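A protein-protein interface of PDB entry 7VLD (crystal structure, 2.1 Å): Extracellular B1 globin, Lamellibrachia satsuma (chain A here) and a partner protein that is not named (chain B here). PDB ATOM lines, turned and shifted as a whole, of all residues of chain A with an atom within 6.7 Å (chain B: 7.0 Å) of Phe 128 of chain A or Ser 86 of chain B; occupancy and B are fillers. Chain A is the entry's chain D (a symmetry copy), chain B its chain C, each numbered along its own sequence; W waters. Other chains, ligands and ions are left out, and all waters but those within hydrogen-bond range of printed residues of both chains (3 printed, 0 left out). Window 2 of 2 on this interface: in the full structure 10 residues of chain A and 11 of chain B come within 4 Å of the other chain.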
ATOM      1  N   GLN A  15      -4.478 -32.298 -13.993  1.00  0.00           N
ATOM      2  CA  GLN A  15      -3.917 -31.757 -12.759  1.00  0.00           C
ATOM      3  C   GLN A  15      -3.944 -32.780 -11.631  1.00  0.00           C
ATOM      4  O   GLN A  15      -3.034 -32.797 -10.794  1.00  0.00           O
ATOM      5  CB  GLN A  15      -4.668 -30.487 -12.353  1.00  0.00           C
ATOM      6  CG  GLN A  15      -4.442 -29.317 -13.300  1.00  0.00           C
ATOM      7  CD  GLN A  15      -4.951 -28.001 -12.745  1.00  0.00           C
ATOM      8  OE1 GLN A  15      -5.758 -27.974 -11.815  1.00  0.00           O
ATOM      9  NE2 GLN A  15      -4.477 -26.898 -13.312  1.00  0.00           N
ATOM     10  N   LEU A 117     -10.412 -29.873   0.194  1.00  0.00           N
ATOM     11  CA  LEU A 117      -9.772 -30.176  -1.082  1.00  0.00           C
ATOM     12  C   LEU A 117      -9.403 -28.900  -1.829  1.00  0.00           C
ATOM     13  O   LEU A 117      -8.296 -28.785  -2.367  1.00  0.00           O
ATOM     14  CB  LEU A 117     -10.690 -31.056  -1.930  1.00  0.00           C
ATOM     15  CG  LEU A 117     -10.890 -32.491  -1.434  1.00  0.00           C
ATOM     16  CD1 LEU A 117     -12.002 -33.189  -2.200  1.00  0.00           C
ATOM     17  CD2 LEU A 117      -9.591 -33.269  -1.556  1.00  0.00           C
ATOM     18  N   MET A 118     -10.313 -27.923  -1.862  1.00  0.00           N
ATOM     19  CA  MET A 118     -10.021 -26.657  -2.524  1.00  0.00           C
ATOM     20  C   MET A 118      -8.873 -25.908  -1.861  1.00  0.00           C
ATOM     21  O   MET A 118      -8.256 -25.048  -2.497  1.00  0.00           O
ATOM     22  CB  MET A 118     -11.271 -25.775  -2.551  1.00  0.00           C
ATOM     23  CG  MET A 118     -12.413 -26.313  -3.403  1.00  0.00           C
ATOM     24  SD  MET A 118     -12.035 -26.375  -5.167  1.00  0.00           S
ATOM     25  CE  MET A 118     -11.684 -28.116  -5.388  1.00  0.00           C
ATOM     26  N   THR A 119      -8.570 -26.217  -0.600  1.00  0.00           N
ATOM     27  CA  THR A 119      -7.465 -25.580   0.108  1.00  0.00           C
ATOM     28  C   THR A 119      -6.158 -26.348  -0.052  1.00  0.00           C
ATOM     29  O   THR A 119      -5.103 -25.738  -0.262  1.00  0.00           O
ATOM     30  CB  THR A 119      -7.809 -25.439   1.596  1.00  0.00           C
ATOM     31  OG1 THR A 119      -9.006 -24.664   1.741  1.00  0.00           O
ATOM     32  CG2 THR A 119      -6.677 -24.754   2.349  1.00  0.00           C
ATOM     33  N   LEU A 121      -5.310 -28.872  -2.377  1.00  0.00           N
ATOM     34  CA  LEU A 121      -4.842 -29.178  -3.729  1.00  0.00           C
ATOM     35  C   LEU A 121      -3.968 -28.095  -4.351  1.00  0.00           C
ATOM     36  O   LEU A 121      -2.960 -28.459  -4.992  1.00  0.00           O
ATOM     37  CB  LEU A 121      -6.046 -29.488  -4.628  1.00  0.00           C
ATOM     38  CG  LEU A 121      -6.748 -30.810  -4.317  1.00  0.00           C
ATOM     39  CD1 LEU A 121      -7.933 -31.022  -5.240  1.00  0.00           C
ATOM     40  CD2 LEU A 121      -5.770 -31.970  -4.416  1.00  0.00           C
ATOM     41  N   PRO A 122      -4.259 -26.795  -4.234  1.00  0.00           N
ATOM     42  CA  PRO A 122      -3.336 -25.799  -4.809  1.00  0.00           C
ATOM     43  C   PRO A 122      -1.936 -25.855  -4.222  1.00  0.00           C
ATOM     44  O   PRO A 122      -0.979 -25.444  -4.892  1.00  0.00           O
ATOM     45  CB  PRO A 122      -4.024 -24.460  -4.505  1.00  0.00           C
ATOM     46  CG  PRO A 122      -5.019 -24.758  -3.437  1.00  0.00           C
ATOM     47  CD  PRO A 122      -5.478 -26.152  -3.711  1.00  0.00           C
ATOM     48  N   SER A 123      -1.780 -26.350  -2.993  1.00  0.00           N
ATOM     49  CA  SER A 123      -0.449 -26.527  -2.424  1.00  0.00           C
ATOM     50  C   SER A 123       0.329 -27.652  -3.091  1.00  0.00           C
ATOM     51  O   SER A 123       1.549 -27.731  -2.908  1.00  0.00           O
ATOM     52  CB  SER A 123      -0.548 -26.799  -0.921  1.00  0.00           C
ATOM     53  OG  SER A 123      -1.306 -25.799  -0.264  1.00  0.00           O
ATOM     54  N   ILE A 125      -0.564 -28.872  -6.627  1.00  0.00           N
ATOM     55  CA  ILE A 125      -0.766 -28.918  -8.071  1.00  0.00           C
ATOM     56  C   ILE A 125      -0.217 -27.645  -8.702  1.00  0.00           C
ATOM     57  O   ILE A 125      -0.410 -26.543  -8.175  1.00  0.00           O
ATOM     58  CB  ILE A 125      -2.262 -29.105  -8.400  1.00  0.00           C
ATOM     59  CG1 ILE A 125      -2.719 -30.512  -8.001  1.00  0.00           C
ATOM     60  CG2 ILE A 125      -2.543 -28.827  -9.870  1.00  0.00           C
ATOM     61  CD1 ILE A 125      -4.214 -30.729  -8.104  1.00  0.00           C
ATOM     62  N   ASP A 126       0.481 -27.801  -9.828  1.00  0.00           N
ATOM     63  CA  ASP A 126       0.932 -26.653 -10.603  1.00  0.00           C
ATOM     64  C   ASP A 126      -0.251 -25.991 -11.298  1.00  0.00           C
ATOM     65  O   ASP A 126      -1.010 -26.654 -12.012  1.00  0.00           O
ATOM     66  CB  ASP A 126       1.964 -27.078 -11.648  1.00  0.00           C
ATOM     67  CG  ASP A 126       3.284 -27.487 -11.036  1.00  0.00           C
ATOM     68  OD1 ASP A 126       3.526 -27.160  -9.857  1.00  0.00           O
ATOM     69  OD2 ASP A 126       4.086 -28.131 -11.745  1.00  0.00           O
ATOM     70  N   ASN A 127      -0.398 -24.681 -11.096  1.00  0.00           N
ATOM     71  CA  ASN A 127      -1.448 -23.895 -11.746  1.00  0.00           C
ATOM     72  C   ASN A 127      -2.832 -24.465 -11.453  1.00  0.00           C
ATOM     73  O   ASN A 127      -3.619 -24.736 -12.364  1.00  0.00           O
ATOM     74  CB  ASN A 127      -1.219 -23.806 -13.257  1.00  0.00           C
ATOM     75  CG  ASN A 127      -0.341 -22.648 -13.646  1.00  0.00           C
ATOM     76  OD1 ASN A 127       0.533 -22.783 -14.497  1.00  0.00           O
ATOM     77  ND2 ASN A 127      -0.570 -21.494 -13.030  1.00  0.00           N
ATOM     78  N   PHE A 128      -3.124 -24.660 -10.168  1.00  0.00           N
ATOM     79  CA  PHE A 128      -4.429 -25.175  -9.780  1.00  0.00           C
ATOM     80  C   PHE A 128      -5.529 -24.289 -10.350  1.00  0.00           C
ATOM     81  O   PHE A 128      -5.486 -23.063 -10.218  1.00  0.00           O
ATOM     82  CB  PHE A 128      -4.542 -25.254  -8.258  1.00  0.00           C
ATOM     83  CG  PHE A 128      -5.859 -25.795  -7.774  1.00  0.00           C
ATOM     84  CD1 PHE A 128      -6.140 -27.150  -7.853  1.00  0.00           C
ATOM     85  CD2 PHE A 128      -6.813 -24.950  -7.231  1.00  0.00           C
ATOM     86  CE1 PHE A 128      -7.349 -27.651  -7.408  1.00  0.00           C
ATOM     87  CE2 PHE A 128      -8.025 -25.446  -6.783  1.00  0.00           C
ATOM     88  CZ  PHE A 128      -8.294 -26.797  -6.872  1.00  0.00           C
ATOM     89  N   ASN A 129      -6.495 -24.914 -11.017  1.00  0.00           N
ATOM     90  CA  ASN A 129      -7.607 -24.199 -11.627  1.00  0.00           C
ATOM     91  C   ASN A 129      -8.840 -24.353 -10.748  1.00  0.00           C
ATOM     92  O   ASN A 129      -9.587 -25.330 -10.894  1.00  0.00           O
ATOM     93  CB  ASN A 129      -7.868 -24.724 -13.044  1.00  0.00           C
ATOM     94  CG  ASN A 129      -8.875 -23.883 -13.813  1.00  0.00           C
ATOM     95  OD1 ASN A 129      -9.905 -23.475 -13.278  1.00  0.00           O
ATOM     96  ND2 ASN A 129      -8.581 -23.628 -15.083  1.00  0.00           N
ATOM     97  N   PRO A 130      -9.093 -23.413  -9.834  1.00  0.00           N
ATOM     98  CA  PRO A 130     -10.244 -23.563  -8.932  1.00  0.00           C
ATOM     99  C   PRO A 130     -11.584 -23.525  -9.644  1.00  0.00           C
ATOM    100  O   PRO A 130     -12.576 -24.004  -9.084  1.00  0.00           O
ATOM    101  CB  PRO A 130     -10.088 -22.381  -7.967  1.00  0.00           C
ATOM    102  CG  PRO A 130      -9.345 -21.360  -8.757  1.00  0.00           C
ATOM    103  CD  PRO A 130      -8.394 -22.132  -9.630  1.00  0.00           C
ATOM    104  N   ASP A 131     -11.650 -22.972 -10.856  1.00  0.00           N
ATOM    105  CA  ASP A 131     -12.911 -22.943 -11.589  1.00  0.00           C
ATOM    106  C   ASP A 131     -13.234 -24.305 -12.191  1.00  0.00           C
ATOM    107  O   ASP A 131     -14.330 -24.837 -11.985  1.00  0.00           O
ATOM    108  CB  ASP A 131     -12.865 -21.873 -12.682  1.00  0.00           C
ATOM    109  CG  ASP A 131     -13.164 -20.482 -12.151  1.00  0.00           C
ATOM    110  OD1 ASP A 131     -13.392 -20.342 -10.931  1.00  0.00           O
ATOM    111  OD2 ASP A 131     -13.174 -19.526 -12.957  1.00  0.00           O
ATOM    112  N   TRP A 133     -11.980 -27.169 -11.336  1.00  0.00           N
ATOM    113  CA  TRP A 133     -12.178 -28.110 -10.237  1.00  0.00           C
ATOM    114  C   TRP A 133     -13.543 -27.925  -9.589  1.00  0.00           C
ATOM    115  O   TRP A 133     -14.219 -28.910  -9.271  1.00  0.00           O
ATOM    116  CB  TRP A 133     -11.059 -27.955  -9.207  1.00  0.00           C
ATOM    117  CG  TRP A 133      -9.839 -28.747  -9.558  1.00  0.00           C
ATOM    118  CD1 TRP A 133      -8.803 -28.353 -10.352  1.00  0.00           C
ATOM    119  CD2 TRP A 133      -9.537 -30.083  -9.138  1.00  0.00           C
ATOM    120  NE1 TRP A 133      -7.871 -29.356 -10.447  1.00  0.00           N
ATOM    121  CE2 TRP A 133      -8.298 -30.429  -9.711  1.00  0.00           C
ATOM    122  CE3 TRP A 133     -10.192 -31.015  -8.329  1.00  0.00           C
ATOM    123  CZ2 TRP A 133      -7.701 -31.671  -9.501  1.00  0.00           C
ATOM    124  CZ3 TRP A 133      -9.598 -32.248  -8.124  1.00  0.00           C
ATOM    125  CH2 TRP A 133      -8.365 -32.564  -8.706  1.00  0.00           C
ATOM    126  N   ARG A 134     -13.973 -26.676  -9.398  1.00  0.00           N
ATOM    127  CA  ARG A 134     -15.289 -26.432  -8.818  1.00  0.00           C
ATOM    128  C   ARG A 134     -16.395 -26.966  -9.720  1.00  0.00           C
ATOM    129  O   ARG A 134     -17.361 -27.571  -9.242  1.00  0.00           O
ATOM    130  CB  ARG A 134     -15.481 -24.938  -8.563  1.00  0.00           C
ATOM    131  CG  ARG A 134     -16.655 -24.596  -7.666  1.00  0.00           C
ATOM    132  CD  ARG A 134     -16.723 -23.098  -7.416  1.00  0.00           C
ATOM    133  NE  ARG A 134     -15.406 -22.544  -7.108  1.00  0.00           N
ATOM    134  CZ  ARG A 134     -14.872 -22.512  -5.891  1.00  0.00           C
ATOM    135  NH1 ARG A 134     -13.669 -21.988  -5.709  1.00  0.00           N
ATOM    136  NH2 ARG A 134     -15.540 -23.004  -4.857  1.00  0.00           N
ATOM    137  N   LEU B  81      -8.406 -12.897 -17.553  1.00  0.00           N
ATOM    138  CA  LEU B  81      -8.052 -13.709 -16.395  1.00  0.00           C
ATOM    139  C   LEU B  81      -8.975 -14.905 -16.201  1.00  0.00           C
ATOM    140  O   LEU B  81      -8.754 -15.686 -15.270  1.00  0.00           O
ATOM    141  CB  LEU B  81      -8.041 -12.849 -15.129  1.00  0.00           C
ATOM    142  CG  LEU B  81      -6.816 -11.948 -14.953  1.00  0.00           C
ATOM    143  CD1 LEU B  81      -6.965 -11.073 -13.718  1.00  0.00           C
ATOM    144  CD2 LEU B  81      -5.544 -12.779 -14.877  1.00  0.00           C
ATOM    145  N   SER B  83      -8.753 -17.298 -18.005  1.00  0.00           N
ATOM    146  CA  SER B  83      -7.803 -18.373 -18.267  1.00  0.00           C
ATOM    147  C   SER B  83      -6.988 -18.743 -17.034  1.00  0.00           C
ATOM    148  O   SER B  83      -6.432 -19.845 -16.986  1.00  0.00           O
ATOM    149  CB  SER B  83      -6.863 -17.973 -19.407  1.00  0.00           C
ATOM    150  OG  SER B  83      -7.582 -17.740 -20.606  1.00  0.00           O
ATOM    151  N   ASP B  84      -6.901 -17.854 -16.044  1.00  0.00           N
ATOM    152  CA  ASP B  84      -6.158 -18.095 -14.807  1.00  0.00           C
ATOM    153  C   ASP B  84      -7.056 -17.709 -13.638  1.00  0.00           C
ATOM    154  O   ASP B  84      -6.914 -16.620 -13.063  1.00  0.00           O
ATOM    155  CB  ASP B  84      -4.848 -17.307 -14.790  1.00  0.00           C
ATOM    156  CG  ASP B  84      -4.004 -17.597 -13.563  1.00  0.00           C
ATOM    157  OD1 ASP B  84      -4.232 -18.636 -12.908  1.00  0.00           O
ATOM    158  OD2 ASP B  84      -3.112 -16.780 -13.251  1.00  0.00           O
ATOM    159  N   PRO B  85      -7.993 -18.582 -13.255  1.00  0.00           N
ATOM    160  CA  PRO B  85      -8.982 -18.203 -12.230  1.00  0.00           C
ATOM    161  C   PRO B  85      -8.402 -17.943 -10.849  1.00  0.00           C
ATOM    162  O   PRO B  85      -9.051 -17.248 -10.056  1.00  0.00           O
ATOM    163  CB  PRO B  85      -9.946 -19.396 -12.212  1.00  0.00           C
ATOM    164  CG  PRO B  85      -9.167 -20.525 -12.777  1.00  0.00           C
ATOM    165  CD  PRO B  85      -8.235 -19.934 -13.786  1.00  0.00           C
ATOM    166  N   SER B  86      -7.223 -18.478 -10.523  1.00  0.00           N
ATOM    167  CA  SER B  86      -6.600 -18.145  -9.244  1.00  0.00           C
ATOM    168  C   SER B  86      -6.328 -16.649  -9.147  1.00  0.00           C
ATOM    169  O   SER B  86      -6.701 -15.999  -8.164  1.00  0.00           O
ATOM    170  CB  SER B  86      -5.308 -18.941  -9.060  1.00  0.00           C
ATOM    171  OG  SER B  86      -5.586 -20.286  -8.715  1.00  0.00           O
ATOM    172  N   THR B  87      -5.676 -16.086 -10.165  1.00  0.00           N
ATOM    173  CA  THR B  87      -5.462 -14.645 -10.195  1.00  0.00           C
ATOM    174  C   THR B  87      -6.773 -13.893 -10.384  1.00  0.00           C
ATOM    175  O   THR B  87      -6.948 -12.807  -9.818  1.00  0.00           O
ATOM    176  CB  THR B  87      -4.473 -14.289 -11.305  1.00  0.00           C
ATOM    177  OG1 THR B  87      -3.278 -15.062 -11.142  1.00  0.00           O
ATOM    178  CG2 THR B  87      -4.118 -12.810 -11.261  1.00  0.00           C
ATOM    179  N   LEU B  88      -7.703 -14.460 -11.158  1.00  0.00           N
ATOM    180  CA  LEU B  88      -9.010 -13.835 -11.343  1.00  0.00           C
ATOM    181  C   LEU B  88      -9.711 -13.614 -10.009  1.00  0.00           C
ATOM    182  O   LEU B  88     -10.269 -12.536  -9.766  1.00  0.00           O
ATOM    183  CB  LEU B  88      -9.871 -14.696 -12.266  1.00  0.00           C
ATOM    184  CG  LEU B  88     -11.345 -14.315 -12.402  1.00  0.00           C
ATOM    185  CD1 LEU B  88     -11.503 -13.012 -13.171  1.00  0.00           C
ATOM    186  CD2 LEU B  88     -12.130 -15.436 -13.065  1.00  0.00           C
ATOM    187  N   ASN B  89      -9.688 -14.620  -9.129  1.00  0.00           N
ATOM    188  CA  ASN B  89     -10.324 -14.483  -7.822  1.00  0.00           C
ATOM    189  C   ASN B  89      -9.748 -13.305  -7.044  1.00  0.00           C
ATOM    190  O   ASN B  89     -10.486 -12.573  -6.375  1.00  0.00           O
ATOM    191  CB  ASN B  89     -10.176 -15.780  -7.025  1.00  0.00           C
ATOM    192  CG  ASN B  89     -11.112 -16.876  -7.508  1.00  0.00           C
ATOM    193  OD1 ASN B  89     -12.184 -16.598  -8.043  1.00  0.00           O
ATOM    194  ND2 ASN B  89     -10.710 -18.127  -7.313  1.00  0.00           N
ATOM    195  N   GLU B  90      -8.431 -13.102  -7.125  1.00  0.00           N
ATOM    196  CA  GLU B  90      -7.826 -11.951  -6.464  1.00  0.00           C
ATOM    197  C   GLU B  90      -8.281 -10.646  -7.104  1.00  0.00           C
ATOM    198  O   GLU B  90      -8.569  -9.670  -6.401  1.00  0.00           O
ATOM    199  CB  GLU B  90      -6.302 -12.063  -6.501  1.00  0.00           C
ATOM    200  CG  GLU B  90      -5.762 -13.262  -5.749  1.00  0.00           C
ATOM    201  CD  GLU B  90      -6.169 -13.256  -4.291  1.00  0.00           C
ATOM    202  OE1 GLU B  90      -6.043 -12.196  -3.641  1.00  0.00           O
ATOM    203  OE2 GLU B  90      -6.627 -14.307  -3.796  1.00  0.00           O
ATOM    204  N   GLN B  91      -8.361 -10.608  -8.436  1.00  0.00           N
ATOM    205  CA  GLN B  91      -8.751  -9.375  -9.111  1.00  0.00           C
ATOM    206  C   GLN B  91     -10.218  -9.046  -8.867  1.00  0.00           C
ATOM    207  O   GLN B  91     -10.575  -7.874  -8.697  1.00  0.00           O
ATOM    208  CB  GLN B  91      -8.459  -9.481 -10.609  1.00  0.00           C
ATOM    209  CG  GLN B  91      -8.919  -8.278 -11.428  1.00  0.00           C
ATOM    210  CD  GLN B  91      -8.229  -6.981 -11.032  1.00  0.00           C
ATOM    211  OE1 GLN B  91      -7.248  -6.979 -10.287  1.00  0.00           O
ATOM    212  NE2 GLN B  91      -8.743  -5.867 -11.539  1.00  0.00           N
ATOM    213  N   ARG B 139     -20.387 -15.218 -13.990  1.00  0.00           N
ATOM    214  CA  ARG B 139     -19.257 -15.703 -13.202  1.00  0.00           C
ATOM    215  C   ARG B 139     -18.388 -14.547 -12.727  1.00  0.00           C
ATOM    216  O   ARG B 139     -17.921 -14.538 -11.582  1.00  0.00           O
ATOM    217  CB  ARG B 139     -18.432 -16.693 -14.027  1.00  0.00           C
ATOM    218  CG  ARG B 139     -16.999 -16.893 -13.541  1.00  0.00           C
ATOM    219  CD  ARG B 139     -16.956 -17.606 -12.198  1.00  0.00           C
ATOM    220  NE  ARG B 139     -15.589 -17.834 -11.736  1.00  0.00           N
ATOM    221  CZ  ARG B 139     -14.959 -17.068 -10.851  1.00  0.00           C
ATOM    222  NH1 ARG B 139     -15.572 -16.016 -10.324  1.00  0.00           N
ATOM    223  NH2 ARG B 139     -13.716 -17.354 -10.488  1.00  0.00           N
HETATM  224  O   HOH W   1     -12.838 -19.743  -7.892  1.00  0.00           O
HETATM  225  O   HOH W   2      -3.133 -21.533  -9.194  1.00  0.00           O
HETATM  226  O   HOH W   3      -5.516 -20.636 -11.912  1.00  0.00           O
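Hydrophobic or aromatic side chains of chain B within 4 Å of the printed part of chain A: Pro 85.
Of the 16 printed residues of chain A, 4 touch a printed residue of chain B.
Among the printed residues, 7 pairs touch across the chains.
Among the printed residues, Asp or Glu carboxylates within 4 Å of a Lys or Arg side-chain nitrogen of the other chain: Asp 131 of chain A with Arg 139 of chain B.
Among the printed residues, pairs that only touch across the chains: Asn 129 of chain A with Pro 85 of chain B (3.1 Å), Asp 131 of chain A with Pro 85 of chain B (3.3 Å), Pro 130 of chain A with Ser 86 of chain B (3.5 Å), Pro 130 of chain A with Pro 85 of chain B (3.6 Å) and Pro 130 of chain A with Asn 89 of chain B (3.8 Å).
OE1 of Gln 15 of chain A lies within hydrogen-bond range of N of Asn 129 of chain A (3.2 Å).
OD1 of Asn 89 of chain B is in hydrogen-bond range of NH2 of Arg 139 of chain B, at 3.0 Å.
The side-chain amide nitrogen (ND2) of Asn 89 of chain B lies close to the backbone carbonyl oxygen (O) of Pro 85 of chain B, 3.3 Å away.
The side-chain amide oxygen (OD1) of Asn 129 of chain A sits at hydrogen-bond distance from the backbone NH (N) of Asp 131 of chain A, at 3.0 Å.
Water W3 lies within hydrogen-bond range of the side-chain carboxylate of Asp 84 of chain B (2.6 Å), the backbone carbonyl oxygen of Phe 128 of chain A (3.0 Å) and the backbone NH of Ser 86 of chain B (3.1 Å).
Water W1 lies within hydrogen-bond range of the side-chain amide nitrogen of Asn 89 of chain B (2.7 Å), the side-chain carboxylate of Asp 131 of chain A (3.1 Å) and the guanidinium group of Arg 134 of chain A (3.2 Å).
Water W2 bridges the side-chain hydroxyl of Ser 86 of chain B and the backbone carbonyl oxygen of Phe 128 of chain A.
Phe 128 of chain A touches just one residue of chain B: Ser 86.
Printed residues of chain A within 4 Å of Asn 89 of chain B: Pro 130.
Printed residues of chain B within 4 Å of Asn 129 of chain A: Pro 85 (3.1 Å).
Printed residues of chain B within 4 Å of Pro 130 of chain A: Pro 85, Ser 86 and Asn 89.
Ser 83 of chain B touches none of the printed residues of chain A.
The nearest residue of chain A that does not touch Ser 86 of chain B is Asn 129 of chain A (5.2 Å).
The nearest printed residue of chain B that does not touch Asp 131 of chain A is Leu 88 of chain B (4.2 Å).
The guanidinium group (NH2) of Arg 139 of chain B is in salt-bridge range of the side-chain carboxylate (OD1) of Asp 131 of chain A (3.0 Å).
The side-chain hydroxyl (OG) of Ser 86 of chain B lies within hydrogen-bond range of the backbone carbonyl oxygen (O) of Phe 128 of chain A (3.2 Å).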
